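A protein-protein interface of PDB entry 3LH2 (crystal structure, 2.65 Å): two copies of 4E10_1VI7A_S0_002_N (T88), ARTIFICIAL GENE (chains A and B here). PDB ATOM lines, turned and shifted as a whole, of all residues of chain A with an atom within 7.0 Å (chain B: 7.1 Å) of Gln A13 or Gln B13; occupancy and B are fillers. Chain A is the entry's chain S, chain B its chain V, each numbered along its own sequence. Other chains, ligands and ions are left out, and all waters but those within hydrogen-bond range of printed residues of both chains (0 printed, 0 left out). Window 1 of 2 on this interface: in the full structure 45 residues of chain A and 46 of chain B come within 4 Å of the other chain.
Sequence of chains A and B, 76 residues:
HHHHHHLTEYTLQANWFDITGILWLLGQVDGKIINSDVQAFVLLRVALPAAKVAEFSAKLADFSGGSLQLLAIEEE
The backbone NH of Thr A11 is in hydrogen-bond range of the backbone carbonyl oxygen of Leu B71 (3.0 Å). The backbone carbonyl oxygen of Leu B44 is in hydrogen-bond range of the backbone NH of Leu A12 (2.7 Å). The side-chain amide oxygen (OE1) of Gln A13 sits at hydrogen-bond distance from the side-chain amide nitrogen (NE2) of Gln B13 (2.6 Å). The backbone carbonyl oxygen of Ala A14 is in hydrogen-bond range of the backbone NH of Val B42 (2.8 Å). The backbone carbonyl oxygen of Gln A39 is in hydrogen-bond range of the backbone NH of Phe B41, at 2.9 Å. The backbone NH of Phe A41 is in hydrogen-bond range of the backbone carbonyl oxygen of Gln B39 (2.9 Å). The backbone carbonyl oxygen of Ala B14 is in hydrogen-bond range of the backbone NH of Val A42. N of Leu B12 is in hydrogen-bond range of O of Leu A44. The backbone carbonyl oxygen (O) of Thr B11 lies within hydrogen-bond range of the backbone NH (N) of Leu A71, at 3.1 Å.
Leu B44 touches Thr A11 (O to CA, 3.1 Å). O of Gln A13 touches CD1 of Leu B68, at 3.5 Å. Ala A14 touches Phe B41. Ile A19 touches Val B42 (CG1 to CB, 3.7 Å). Ile A22 touches Leu B44 (CG2 to CD2, 3.9 Å). Leu B43 touches Gln A39 (CD1 to CG, 3.6 Å). Val A42 touches Ile B19 (CB to CD1, 3.7 Å). Leu A43 touches Gln B13 (CD2 to CG, 3.6 Å). Leu A68 touches Gln B13. C of Leu A70 touches O of Thr B11 (3.99 Å).
Printed residues of chain B within 4 Å of Gln A13: Gln B13, Phe B41, Val B42, Leu B43 and Leu B68. Gln B13 touches just these residues of chain A: Gln A13, Phe A41, Val A42, Leu A43 and Leu A68. Of the printed residues of chain A, Leu B68 touches Gln A13 (3.5 Å) and Ile A22 (3.7 Å). Of the printed residues of chain B, Thr A11 touches Leu B44 (3.1 Å), Leu B70 (3.8 Å) and Leu B71 (3.0 Å). Of the printed residues of chain A, Ile B19 touches Val A42 and Leu A44. Printed residues of chain A within 4 Å of Leu B12: Val A42, Leu A43, Leu A44, Gln A69 and Leu A70. Asn B15 touches none of the printed residues of chain A. The nearest residue of chain B that does not touch Gln A13 is Leu B44 (5.0 Å). The nearest residue of chain A that does not touch Gln B13 is Gln A69 (4.7 Å). The nearest printed residue of chain B that does not touch Val A42 is Asn B15 (4.9 Å).
Printed residues of chain A that touch a printed residue of chain B: Thr A11, Leu A12, Gln A13, Ala A14, Asn A15, Ile A19, Ile A22, Gln A39, Phe A41, Val A42, Leu A43, Leu A44, Leu A68, Gln A69, Leu A70 and Leu A71. Of the 17 printed residues of chain B, 14 touch a printed residue of chain A. Hydrophobic or aromatic side chains of chain B within 4 Å of the printed part of chain A: Leu B12, Ile B19, Phe B41, Val B42, Leu B43, Leu B44, Leu B68, Leu B70 and Leu B71. Among the printed residues, no Asp or Glu carboxylate lies within 4 Å of a Lys or Arg side-chain nitrogen of the other chain.
Leu A12 touches Val B42, and with the chains exchanged Val A42 touches Leu B12. Gln A13 touches Phe B41, and with the chains exchanged Phe A41 touches Gln B13. Gln A13 touches Leu B43, and with the chains exchanged Leu A43 touches Gln B13. Ile A22 touches Leu B44, but with the chains exchanged Leu A44 does not touch Ile B22 (4.1 Å). 17 positions are printed for both chains.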
ATOM      1  N   THR A  11     -21.587 -11.937 -14.466  1.00  0.00           N
ATOM      2  CA  THR A  11     -21.750 -10.762 -15.312  1.00  0.00           C
ATOM      3  C   THR A  11     -21.316  -9.522 -14.553  1.00  0.00           C
ATOM      4  O   THR A  11     -21.154  -9.545 -13.329  1.00  0.00           O
ATOM      5  CB  THR A  11     -23.202 -10.550 -15.763  1.00  0.00           C
ATOM      6  OG1 THR A  11     -24.063 -10.571 -14.618  1.00  0.00           O
ATOM      7  CG2 THR A  11     -23.625 -11.615 -16.761  1.00  0.00           C
ATOM      8  N   LEU A  12     -21.135  -8.435 -15.288  1.00  0.00           N
ATOM      9  CA  LEU A  12     -20.591  -7.233 -14.711  1.00  0.00           C
ATOM     10  C   LEU A  12     -20.956  -6.032 -15.569  1.00  0.00           C
ATOM     11  O   LEU A  12     -20.905  -6.089 -16.802  1.00  0.00           O
ATOM     12  CB  LEU A  12     -19.071  -7.365 -14.603  1.00  0.00           C
ATOM     13  CG  LEU A  12     -18.374  -6.492 -13.566  1.00  0.00           C
ATOM     14  CD1 LEU A  12     -19.174  -6.428 -12.266  1.00  0.00           C
ATOM     15  CD2 LEU A  12     -16.968  -7.026 -13.320  1.00  0.00           C
ATOM     16  N   GLN A  13     -21.321  -4.943 -14.904  1.00  0.00           N
ATOM     17  CA  GLN A  13     -21.683  -3.717 -15.582  1.00  0.00           C
ATOM     18  C   GLN A  13     -20.744  -2.608 -15.143  1.00  0.00           C
ATOM     19  O   GLN A  13     -20.644  -2.320 -13.958  1.00  0.00           O
ATOM     20  CB  GLN A  13     -23.127  -3.354 -15.240  1.00  0.00           C
ATOM     21  CG  GLN A  13     -23.532  -1.962 -15.665  1.00  0.00           C
ATOM     22  CD  GLN A  13     -25.014  -1.727 -15.537  1.00  0.00           C
ATOM     23  OE1 GLN A  13     -25.442  -0.780 -14.874  1.00  0.00           O
ATOM     24  NE2 GLN A  13     -25.813  -2.585 -16.168  1.00  0.00           N
ATOM     25  N   ALA A  14     -20.048  -1.990 -16.090  1.00  0.00           N
ATOM     26  CA  ALA A  14     -19.182  -0.853 -15.767  1.00  0.00           C
ATOM     27  C   ALA A  14     -19.211   0.212 -16.858  1.00  0.00           C
ATOM     28  O   ALA A  14     -19.561  -0.057 -18.008  1.00  0.00           O
ATOM     29  CB  ALA A  14     -17.740  -1.321 -15.527  1.00  0.00           C
ATOM     30  N   ASN A  15     -18.834   1.429 -16.490  1.00  0.00           N
ATOM     31  CA  ASN A  15     -18.674   2.465 -17.485  1.00  0.00           C
ATOM     32  C   ASN A  15     -17.378   2.178 -18.232  1.00  0.00           C
ATOM     33  O   ASN A  15     -16.496   1.494 -17.725  1.00  0.00           O
ATOM     34  CB  ASN A  15     -18.709   3.868 -16.861  1.00  0.00           C
ATOM     35  CG  ASN A  15     -17.336   4.432 -16.592  1.00  0.00           C
ATOM     36  OD1 ASN A  15     -16.575   4.702 -17.515  1.00  0.00           O
ATOM     37  ND2 ASN A  15     -17.023   4.649 -15.324  1.00  0.00           N
ATOM     38  N   ILE A  19     -13.346  -0.368 -17.608  1.00  0.00           N
ATOM     39  CA  ILE A  19     -13.210  -1.706 -18.140  1.00  0.00           C
ATOM     40  C   ILE A  19     -11.777  -2.193 -18.084  1.00  0.00           C
ATOM     41  O   ILE A  19     -11.534  -3.305 -17.640  1.00  0.00           O
ATOM     42  CB  ILE A  19     -13.756  -1.813 -19.574  1.00  0.00           C
ATOM     43  CG1 ILE A  19     -15.289  -1.777 -19.548  1.00  0.00           C
ATOM     44  CG2 ILE A  19     -13.288  -3.103 -20.231  1.00  0.00           C
ATOM     45  CD1 ILE A  19     -15.923  -2.864 -18.669  1.00  0.00           C
ATOM     46  N   ILE A  22     -10.769  -3.385 -14.758  1.00  0.00           N
ATOM     47  CA  ILE A  22     -11.428  -4.653 -14.510  1.00  0.00           C
ATOM     48  C   ILE A  22     -10.648  -5.767 -15.207  1.00  0.00           C
ATOM     49  O   ILE A  22     -10.444  -6.833 -14.638  1.00  0.00           O
ATOM     50  CB  ILE A  22     -12.897  -4.593 -14.969  1.00  0.00           C
ATOM     51  CG1 ILE A  22     -13.668  -3.647 -14.035  1.00  0.00           C
ATOM     52  CG2 ILE A  22     -13.526  -5.983 -14.988  1.00  0.00           C
ATOM     53  CD1 ILE A  22     -15.069  -3.312 -14.485  1.00  0.00           C
ATOM     54  N   GLN A  39     -24.608  -1.475 -23.852  1.00  0.00           N
ATOM     55  CA  GLN A  39     -26.030  -1.262 -23.695  1.00  0.00           C
ATOM     56  C   GLN A  39     -26.260   0.125 -23.131  1.00  0.00           C
ATOM     57  O   GLN A  39     -25.569   0.546 -22.204  1.00  0.00           O
ATOM     58  CB  GLN A  39     -26.618  -2.273 -22.711  1.00  0.00           C
ATOM     59  CG  GLN A  39     -26.429  -3.738 -23.071  1.00  0.00           C
ATOM     60  CD  GLN A  39     -27.488  -4.273 -24.017  1.00  0.00           C
ATOM     61  OE1 GLN A  39     -28.503  -3.620 -24.274  1.00  0.00           O
ATOM     62  NE2 GLN A  39     -27.263  -5.480 -24.526  1.00  0.00           N
ATOM     63  N   PHE A  41     -29.023   2.517 -21.120  1.00  0.00           N
ATOM     64  CA  PHE A  41     -30.109   2.362 -20.172  1.00  0.00           C
ATOM     65  C   PHE A  41     -30.649   3.722 -19.793  1.00  0.00           C
ATOM     66  O   PHE A  41     -29.972   4.736 -19.946  1.00  0.00           O
ATOM     67  CB  PHE A  41     -29.619   1.670 -18.906  1.00  0.00           C
ATOM     68  CG  PHE A  41     -29.160   0.257 -19.123  1.00  0.00           C
ATOM     69  CD1 PHE A  41     -27.829  -0.023 -19.369  1.00  0.00           C
ATOM     70  CD2 PHE A  41     -30.057  -0.791 -19.084  1.00  0.00           C
ATOM     71  CE1 PHE A  41     -27.411  -1.326 -19.569  1.00  0.00           C
ATOM     72  CE2 PHE A  41     -29.635  -2.090 -19.279  1.00  0.00           C
ATOM     73  CZ  PHE A  41     -28.317  -2.354 -19.520  1.00  0.00           C
ATOM     74  N   VAL A  42     -31.879   3.748 -19.307  1.00  0.00           N
ATOM     75  CA  VAL A  42     -32.425   4.964 -18.743  1.00  0.00           C
ATOM     76  C   VAL A  42     -32.328   4.804 -17.238  1.00  0.00           C
ATOM     77  O   VAL A  42     -32.748   3.786 -16.693  1.00  0.00           O
ATOM     78  CB  VAL A  42     -33.895   5.193 -19.174  1.00  0.00           C
ATOM     79  CG1 VAL A  42     -34.469   6.457 -18.524  1.00  0.00           C
ATOM     80  CG2 VAL A  42     -33.985   5.272 -20.687  1.00  0.00           C
ATOM     81  N   LEU A  43     -31.731   5.786 -16.575  1.00  0.00           N
ATOM     82  CA  LEU A  43     -31.667   5.796 -15.122  1.00  0.00           C
ATOM     83  C   LEU A  43     -32.782   6.671 -14.559  1.00  0.00           C
ATOM     84  O   LEU A  43     -32.870   7.858 -14.862  1.00  0.00           O
ATOM     85  CB  LEU A  43     -30.316   6.312 -14.650  1.00  0.00           C
ATOM     86  CG  LEU A  43     -29.087   5.493 -15.034  1.00  0.00           C
ATOM     87  CD1 LEU A  43     -27.895   5.922 -14.176  1.00  0.00           C
ATOM     88  CD2 LEU A  43     -29.344   4.007 -14.888  1.00  0.00           C
ATOM     89  N   LEU A  44     -33.642   6.068 -13.749  1.00  0.00           N
ATOM     90  CA  LEU A  44     -34.740   6.792 -13.126  1.00  0.00           C
ATOM     91  C   LEU A  44     -34.467   6.982 -11.639  1.00  0.00           C
ATOM     92  O   LEU A  44     -33.996   6.059 -10.966  1.00  0.00           O
ATOM     93  CB  LEU A  44     -36.053   6.027 -13.317  1.00  0.00           C
ATOM     94  CG  LEU A  44     -37.011   6.441 -14.439  1.00  0.00           C
ATOM     95  CD1 LEU A  44     -36.328   7.198 -15.569  1.00  0.00           C
ATOM     96  CD2 LEU A  44     -37.728   5.214 -14.969  1.00  0.00           C
ATOM     97  N   SER A  67     -35.869  -9.242 -13.134  1.00  0.00           N
ATOM     98  CA  SER A  67     -34.642  -8.583 -13.597  1.00  0.00           C
ATOM     99  C   SER A  67     -34.494  -7.117 -13.176  1.00  0.00           C
ATOM    100  O   SER A  67     -33.419  -6.533 -13.332  1.00  0.00           O
ATOM    101  CB  SER A  67     -34.540  -8.682 -15.124  1.00  0.00           C
ATOM    102  OG  SER A  67     -35.440  -7.791 -15.759  1.00  0.00           O
ATOM    103  N   LEU A  68     -35.559  -6.521 -12.651  1.00  0.00           N
ATOM    104  CA  LEU A  68     -35.528  -5.106 -12.291  1.00  0.00           C
ATOM    105  C   LEU A  68     -35.256  -4.973 -10.799  1.00  0.00           C
ATOM    106  O   LEU A  68     -35.839  -5.694  -9.988  1.00  0.00           O
ATOM    107  CB  LEU A  68     -36.848  -4.428 -12.662  1.00  0.00           C
ATOM    108  CG  LEU A  68     -36.763  -3.083 -13.390  1.00  0.00           C
ATOM    109  CD1 LEU A  68     -35.988  -3.198 -14.698  1.00  0.00           C
ATOM    110  CD2 LEU A  68     -38.164  -2.552 -13.653  1.00  0.00           C
ATOM    111  N   GLN A  69     -34.365  -4.051 -10.445  1.00  0.00           N
ATOM    112  CA  GLN A  69     -33.907  -3.904  -9.068  1.00  0.00           C
ATOM    113  C   GLN A  69     -34.072  -2.463  -8.586  1.00  0.00           C
ATOM    114  O   GLN A  69     -33.536  -1.532  -9.190  1.00  0.00           O
ATOM    115  CB  GLN A  69     -32.433  -4.320  -8.961  1.00  0.00           C
ATOM    116  CG  GLN A  69     -32.078  -5.577  -9.752  1.00  0.00           C
ATOM    117  N   LEU A  70     -34.809  -2.283  -7.494  1.00  0.00           N
ATOM    118  CA  LEU A  70     -34.987  -0.963  -6.901  1.00  0.00           C
ATOM    119  C   LEU A  70     -33.817  -0.677  -5.955  1.00  0.00           C
ATOM    120  O   LEU A  70     -33.514  -1.494  -5.090  1.00  0.00           O
ATOM    121  CB  LEU A  70     -36.316  -0.905  -6.146  1.00  0.00           C
ATOM    122  CG  LEU A  70     -37.049   0.437  -6.183  1.00  0.00           C
ATOM    123  CD1 LEU A  70     -37.399   0.814  -7.607  1.00  0.00           C
ATOM    124  CD2 LEU A  70     -38.304   0.388  -5.330  1.00  0.00           C
ATOM    125  N   LEU A  71     -33.155   0.468  -6.127  1.00  0.00           N
ATOM    126  CA  LEU A  71     -31.991   0.823  -5.304  1.00  0.00           C
ATOM    127  C   LEU A  71     -32.157   2.207  -4.684  1.00  0.00           C
ATOM    128  O   LEU A  71     -32.225   2.348  -3.461  1.00  0.00           O
ATOM    129  CB  LEU A  71     -30.709   0.790  -6.138  1.00  0.00           C
ATOM    130  CG  LEU A  71     -30.583  -0.403  -7.086  1.00  0.00           C
ATOM    131  CD1 LEU A  71     -29.291  -0.337  -7.895  1.00  0.00           C
ATOM    132  CD2 LEU A  71     -30.676  -1.708  -6.299  1.00  0.00           C
ATOM    133  N   THR B  11     -33.437   4.701  -6.922  1.00  0.00           N
ATOM    134  CA  THR B  11     -33.049   4.809  -8.320  1.00  0.00           C
ATOM    135  C   THR B  11     -33.419   3.518  -9.024  1.00  0.00           C
ATOM    136  O   THR B  11     -33.599   2.480  -8.388  1.00  0.00           O
ATOM    137  CB  THR B  11     -31.549   5.036  -8.493  1.00  0.00           C
ATOM    138  OG1 THR B  11     -30.834   3.994  -7.818  1.00  0.00           O
ATOM    139  CG2 THR B  11     -31.140   6.402  -7.945  1.00  0.00           C
ATOM    140  N   LEU B  12     -33.526   3.584 -10.343  1.00  0.00           N
ATOM    141  CA  LEU B  12     -34.016   2.459 -11.111  1.00  0.00           C
ATOM    142  C   LEU B  12     -33.338   2.497 -12.464  1.00  0.00           C
ATOM    143  O   LEU B  12     -33.297   3.546 -13.111  1.00  0.00           O
ATOM    144  CB  LEU B  12     -35.537   2.555 -11.250  1.00  0.00           C
ATOM    145  CG  LEU B  12     -36.363   1.295 -11.501  1.00  0.00           C
ATOM    146  CD1 LEU B  12     -35.690   0.041 -10.976  1.00  0.00           C
ATOM    147  CD2 LEU B  12     -37.733   1.473 -10.870  1.00  0.00           C
ATOM    148  N   GLN B  13     -32.777   1.360 -12.865  1.00  0.00           N
ATOM    149  CA  GLN B  13     -32.089   1.244 -14.140  1.00  0.00           C
ATOM    150  C   GLN B  13     -32.905   0.347 -15.058  1.00  0.00           C
ATOM    151  O   GLN B  13     -33.220  -0.787 -14.711  1.00  0.00           O
ATOM    152  CB  GLN B  13     -30.681   0.666 -13.946  1.00  0.00           C
ATOM    153  CG  GLN B  13     -29.932   0.426 -15.250  1.00  0.00           C
ATOM    154  CD  GLN B  13     -28.573  -0.202 -15.047  1.00  0.00           C
ATOM    155  OE1 GLN B  13     -28.309  -1.304 -15.532  1.00  0.00           O
ATOM    156  NE2 GLN B  13     -27.696   0.496 -14.331  1.00  0.00           N
ATOM    157  N   ALA B  14     -33.258   0.848 -16.232  1.00  0.00           N
ATOM    158  CA  ALA B  14     -34.066   0.048 -17.137  1.00  0.00           C
ATOM    159  C   ALA B  14     -33.825   0.351 -18.601  1.00  0.00           C
ATOM    160  O   ALA B  14     -33.448   1.454 -18.990  1.00  0.00           O
ATOM    161  CB  ALA B  14     -35.549   0.208 -16.808  1.00  0.00           C
ATOM    162  N   ASN B  15     -34.051  -0.674 -19.401  1.00  0.00           N
ATOM    163  CA  ASN B  15     -34.135  -0.538 -20.835  1.00  0.00           C
ATOM    164  C   ASN B  15     -35.233   0.471 -21.178  1.00  0.00           C
ATOM    165  O   ASN B  15     -36.218   0.602 -20.458  1.00  0.00           O
ATOM    166  CB  ASN B  15     -34.361  -1.932 -21.443  1.00  0.00           C
ATOM    167  CG  ASN B  15     -35.453  -1.969 -22.480  1.00  0.00           C
ATOM    168  OD1 ASN B  15     -35.651  -1.028 -23.243  1.00  0.00           O
ATOM    169  ND2 ASN B  15     -36.164  -3.092 -22.531  1.00  0.00           N
ATOM    170  N   ILE B  19     -39.613   1.892 -19.694  1.00  0.00           N
ATOM    171  CA  ILE B  19     -39.783   3.095 -18.895  1.00  0.00           C
ATOM    172  C   ILE B  19     -41.240   3.504 -18.728  1.00  0.00           C
ATOM    173  O   ILE B  19     -41.667   3.763 -17.606  1.00  0.00           O
ATOM    174  CB  ILE B  19     -38.999   4.278 -19.458  1.00  0.00           C
ATOM    175  CG1 ILE B  19     -37.501   4.035 -19.284  1.00  0.00           C
ATOM    176  CG2 ILE B  19     -39.406   5.560 -18.746  1.00  0.00           C
ATOM    177  CD1 ILE B  19     -37.064   3.912 -17.822  1.00  0.00           C
ATOM    178  N   ILE B  22     -42.934   1.526 -16.233  1.00  0.00           N
ATOM    179  CA  ILE B  22     -42.529   1.914 -14.891  1.00  0.00           C
ATOM    180  C   ILE B  22     -43.342   3.137 -14.444  1.00  0.00           C
ATOM    181  O   ILE B  22     -43.872   3.165 -13.331  1.00  0.00           O
ATOM    182  CB  ILE B  22     -41.017   2.196 -14.833  1.00  0.00           C
ATOM    183  CG1 ILE B  22     -40.241   0.901 -15.045  1.00  0.00           C
ATOM    184  CG2 ILE B  22     -40.632   2.796 -13.505  1.00  0.00           C
ATOM    185  CD1 ILE B  22     -38.772   1.119 -15.250  1.00  0.00           C
ATOM    186  N   GLN B  39     -27.489   6.625 -19.850  1.00  0.00           N
ATOM    187  CA  GLN B  39     -26.110   6.183 -19.665  1.00  0.00           C
ATOM    188  C   GLN B  39     -25.823   4.924 -20.458  1.00  0.00           C
ATOM    189  O   GLN B  39     -26.630   3.998 -20.464  1.00  0.00           O
ATOM    190  CB  GLN B  39     -25.864   5.872 -18.201  1.00  0.00           C
ATOM    191  CG  GLN B  39     -25.883   7.073 -17.300  1.00  0.00           C
ATOM    192  CD  GLN B  39     -24.570   7.795 -17.302  1.00  0.00           C
ATOM    193  OE1 GLN B  39     -23.583   7.299 -17.838  1.00  0.00           O
ATOM    194  NE2 GLN B  39     -24.542   8.971 -16.697  1.00  0.00           N
ATOM    195  N   PHE B  41     -23.262   1.647 -20.788  1.00  0.00           N
ATOM    196  CA  PHE B  41     -22.349   0.836 -19.991  1.00  0.00           C
ATOM    197  C   PHE B  41     -21.814  -0.313 -20.829  1.00  0.00           C
ATOM    198  O   PHE B  41     -22.472  -0.765 -21.763  1.00  0.00           O
ATOM    199  CB  PHE B  41     -23.069   0.249 -18.777  1.00  0.00           C
ATOM    200  CG  PHE B  41     -23.595   1.280 -17.810  1.00  0.00           C
ATOM    201  CD1 PHE B  41     -24.921   1.682 -17.856  1.00  0.00           C
ATOM    202  CD2 PHE B  41     -22.769   1.833 -16.842  1.00  0.00           C
ATOM    203  CE1 PHE B  41     -25.413   2.621 -16.961  1.00  0.00           C
ATOM    204  CE2 PHE B  41     -23.259   2.770 -15.949  1.00  0.00           C
ATOM    205  CZ  PHE B  41     -24.586   3.163 -16.012  1.00  0.00           C
ATOM    206  N   VAL B  42     -20.616  -0.785 -20.501  1.00  0.00           N
ATOM    207  CA  VAL B  42     -20.113  -2.019 -21.083  1.00  0.00           C
ATOM    208  C   VAL B  42     -20.560  -3.170 -20.182  1.00  0.00           C
ATOM    209  O   VAL B  42     -20.415  -3.099 -18.965  1.00  0.00           O
ATOM    210  CB  VAL B  42     -18.569  -2.016 -21.197  1.00  0.00           C
ATOM    211  CG1 VAL B  42     -18.074  -3.301 -21.858  1.00  0.00           C
ATOM    212  CG2 VAL B  42     -18.095  -0.809 -21.971  1.00  0.00           C
ATOM    213  N   LEU B  43     -21.130  -4.216 -20.770  1.00  0.00           N
ATOM    214  CA  LEU B  43     -21.449  -5.425 -20.014  1.00  0.00           C
ATOM    215  C   LEU B  43     -20.378  -6.485 -20.250  1.00  0.00           C
ATOM    216  O   LEU B  43     -19.985  -6.747 -21.385  1.00  0.00           O
ATOM    217  CB  LEU B  43     -22.819  -5.981 -20.406  1.00  0.00           C
ATOM    218  CG  LEU B  43     -23.977  -4.992 -20.367  1.00  0.00           C
ATOM    219  CD1 LEU B  43     -25.312  -5.723 -20.311  1.00  0.00           C
ATOM    220  CD2 LEU B  43     -23.831  -4.051 -19.181  1.00  0.00           C
ATOM    221  N   LEU B  44     -19.914  -7.090 -19.166  1.00  0.00           N
ATOM    222  CA  LEU B  44     -18.906  -8.136 -19.230  1.00  0.00           C
ATOM    223  C   LEU B  44     -19.488  -9.423 -18.674  1.00  0.00           C
ATOM    224  O   LEU B  44     -20.172  -9.416 -17.654  1.00  0.00           O
ATOM    225  CB  LEU B  44     -17.671  -7.738 -18.410  1.00  0.00           C
ATOM    226  CG  LEU B  44     -16.430  -7.202 -19.131  1.00  0.00           C
ATOM    227  CD1 LEU B  44     -16.749  -6.544 -20.466  1.00  0.00           C
ATOM    228  CD2 LEU B  44     -15.675  -6.238 -18.227  1.00  0.00           C
ATOM    229  N   SER B  67     -19.114   0.759  -6.040  1.00  0.00           N
ATOM    230  CA  SER B  67     -20.202   0.766  -7.016  1.00  0.00           C
ATOM    231  C   SER B  67     -20.331  -0.594  -7.703  1.00  0.00           C
ATOM    232  O   SER B  67     -21.400  -1.203  -7.681  1.00  0.00           O
ATOM    233  CB  SER B  67     -19.980   1.863  -8.065  1.00  0.00           C
ATOM    234  N   LEU B  68     -19.239  -1.064  -8.302  1.00  0.00           N
ATOM    235  CA  LEU B  68     -19.241  -2.319  -9.061  1.00  0.00           C
ATOM    236  C   LEU B  68     -19.699  -3.518  -8.233  1.00  0.00           C
ATOM    237  O   LEU B  68     -19.199  -3.769  -7.136  1.00  0.00           O
ATOM    238  CB  LEU B  68     -17.852  -2.609  -9.647  1.00  0.00           C
ATOM    239  CG  LEU B  68     -17.561  -2.175 -11.089  1.00  0.00           C
ATOM    240  CD1 LEU B  68     -18.424  -0.991 -11.531  1.00  0.00           C
ATOM    241  CD2 LEU B  68     -16.080  -1.860 -11.242  1.00  0.00           C
ATOM    242  N   GLN B  69     -20.646  -4.258  -8.796  1.00  0.00           N
ATOM    243  CA  GLN B  69     -21.226  -5.420  -8.146  1.00  0.00           C
ATOM    244  C   GLN B  69     -21.166  -6.636  -9.070  1.00  0.00           C
ATOM    245  O   GLN B  69     -21.715  -6.628 -10.172  1.00  0.00           O
ATOM    246  CB  GLN B  69     -22.676  -5.132  -7.738  1.00  0.00           C
ATOM    247  CG  GLN B  69     -23.502  -4.409  -8.797  1.00  0.00           C
ATOM    248  N   LEU B  70     -20.491  -7.681  -8.610  1.00  0.00           N
ATOM    249  CA  LEU B  70     -20.362  -8.908  -9.373  1.00  0.00           C
ATOM    250  C   LEU B  70     -21.607  -9.770  -9.177  1.00  0.00           C
ATOM    251  O   LEU B  70     -21.880 -10.213  -8.071  1.00  0.00           O
ATOM    252  CB  LEU B  70     -19.110  -9.654  -8.919  1.00  0.00           C
ATOM    253  CG  LEU B  70     -18.575 -10.752  -9.828  1.00  0.00           C
ATOM    254  CD1 LEU B  70     -18.151 -10.196 -11.176  1.00  0.00           C
ATOM    255  CD2 LEU B  70     -17.410 -11.431  -9.141  1.00  0.00           C
ATOM    256  N   LEU B  71     -22.361  -9.998 -10.249  1.00  0.00           N
ATOM    257  CA  LEU B  71     -23.611 -10.759 -10.169  1.00  0.00           C
ATOM    258  C   LEU B  71     -23.477 -12.175 -10.739  1.00  0.00           C
ATOM    259  O   LEU B  71     -22.779 -12.397 -11.727  1.00  0.00           O
ATOM    260  CB  LEU B  71     -24.741 -10.011 -10.882  1.00  0.00           C
ATOM    261  CG  LEU B  71     -25.245  -8.757 -10.158  1.00  0.00           C
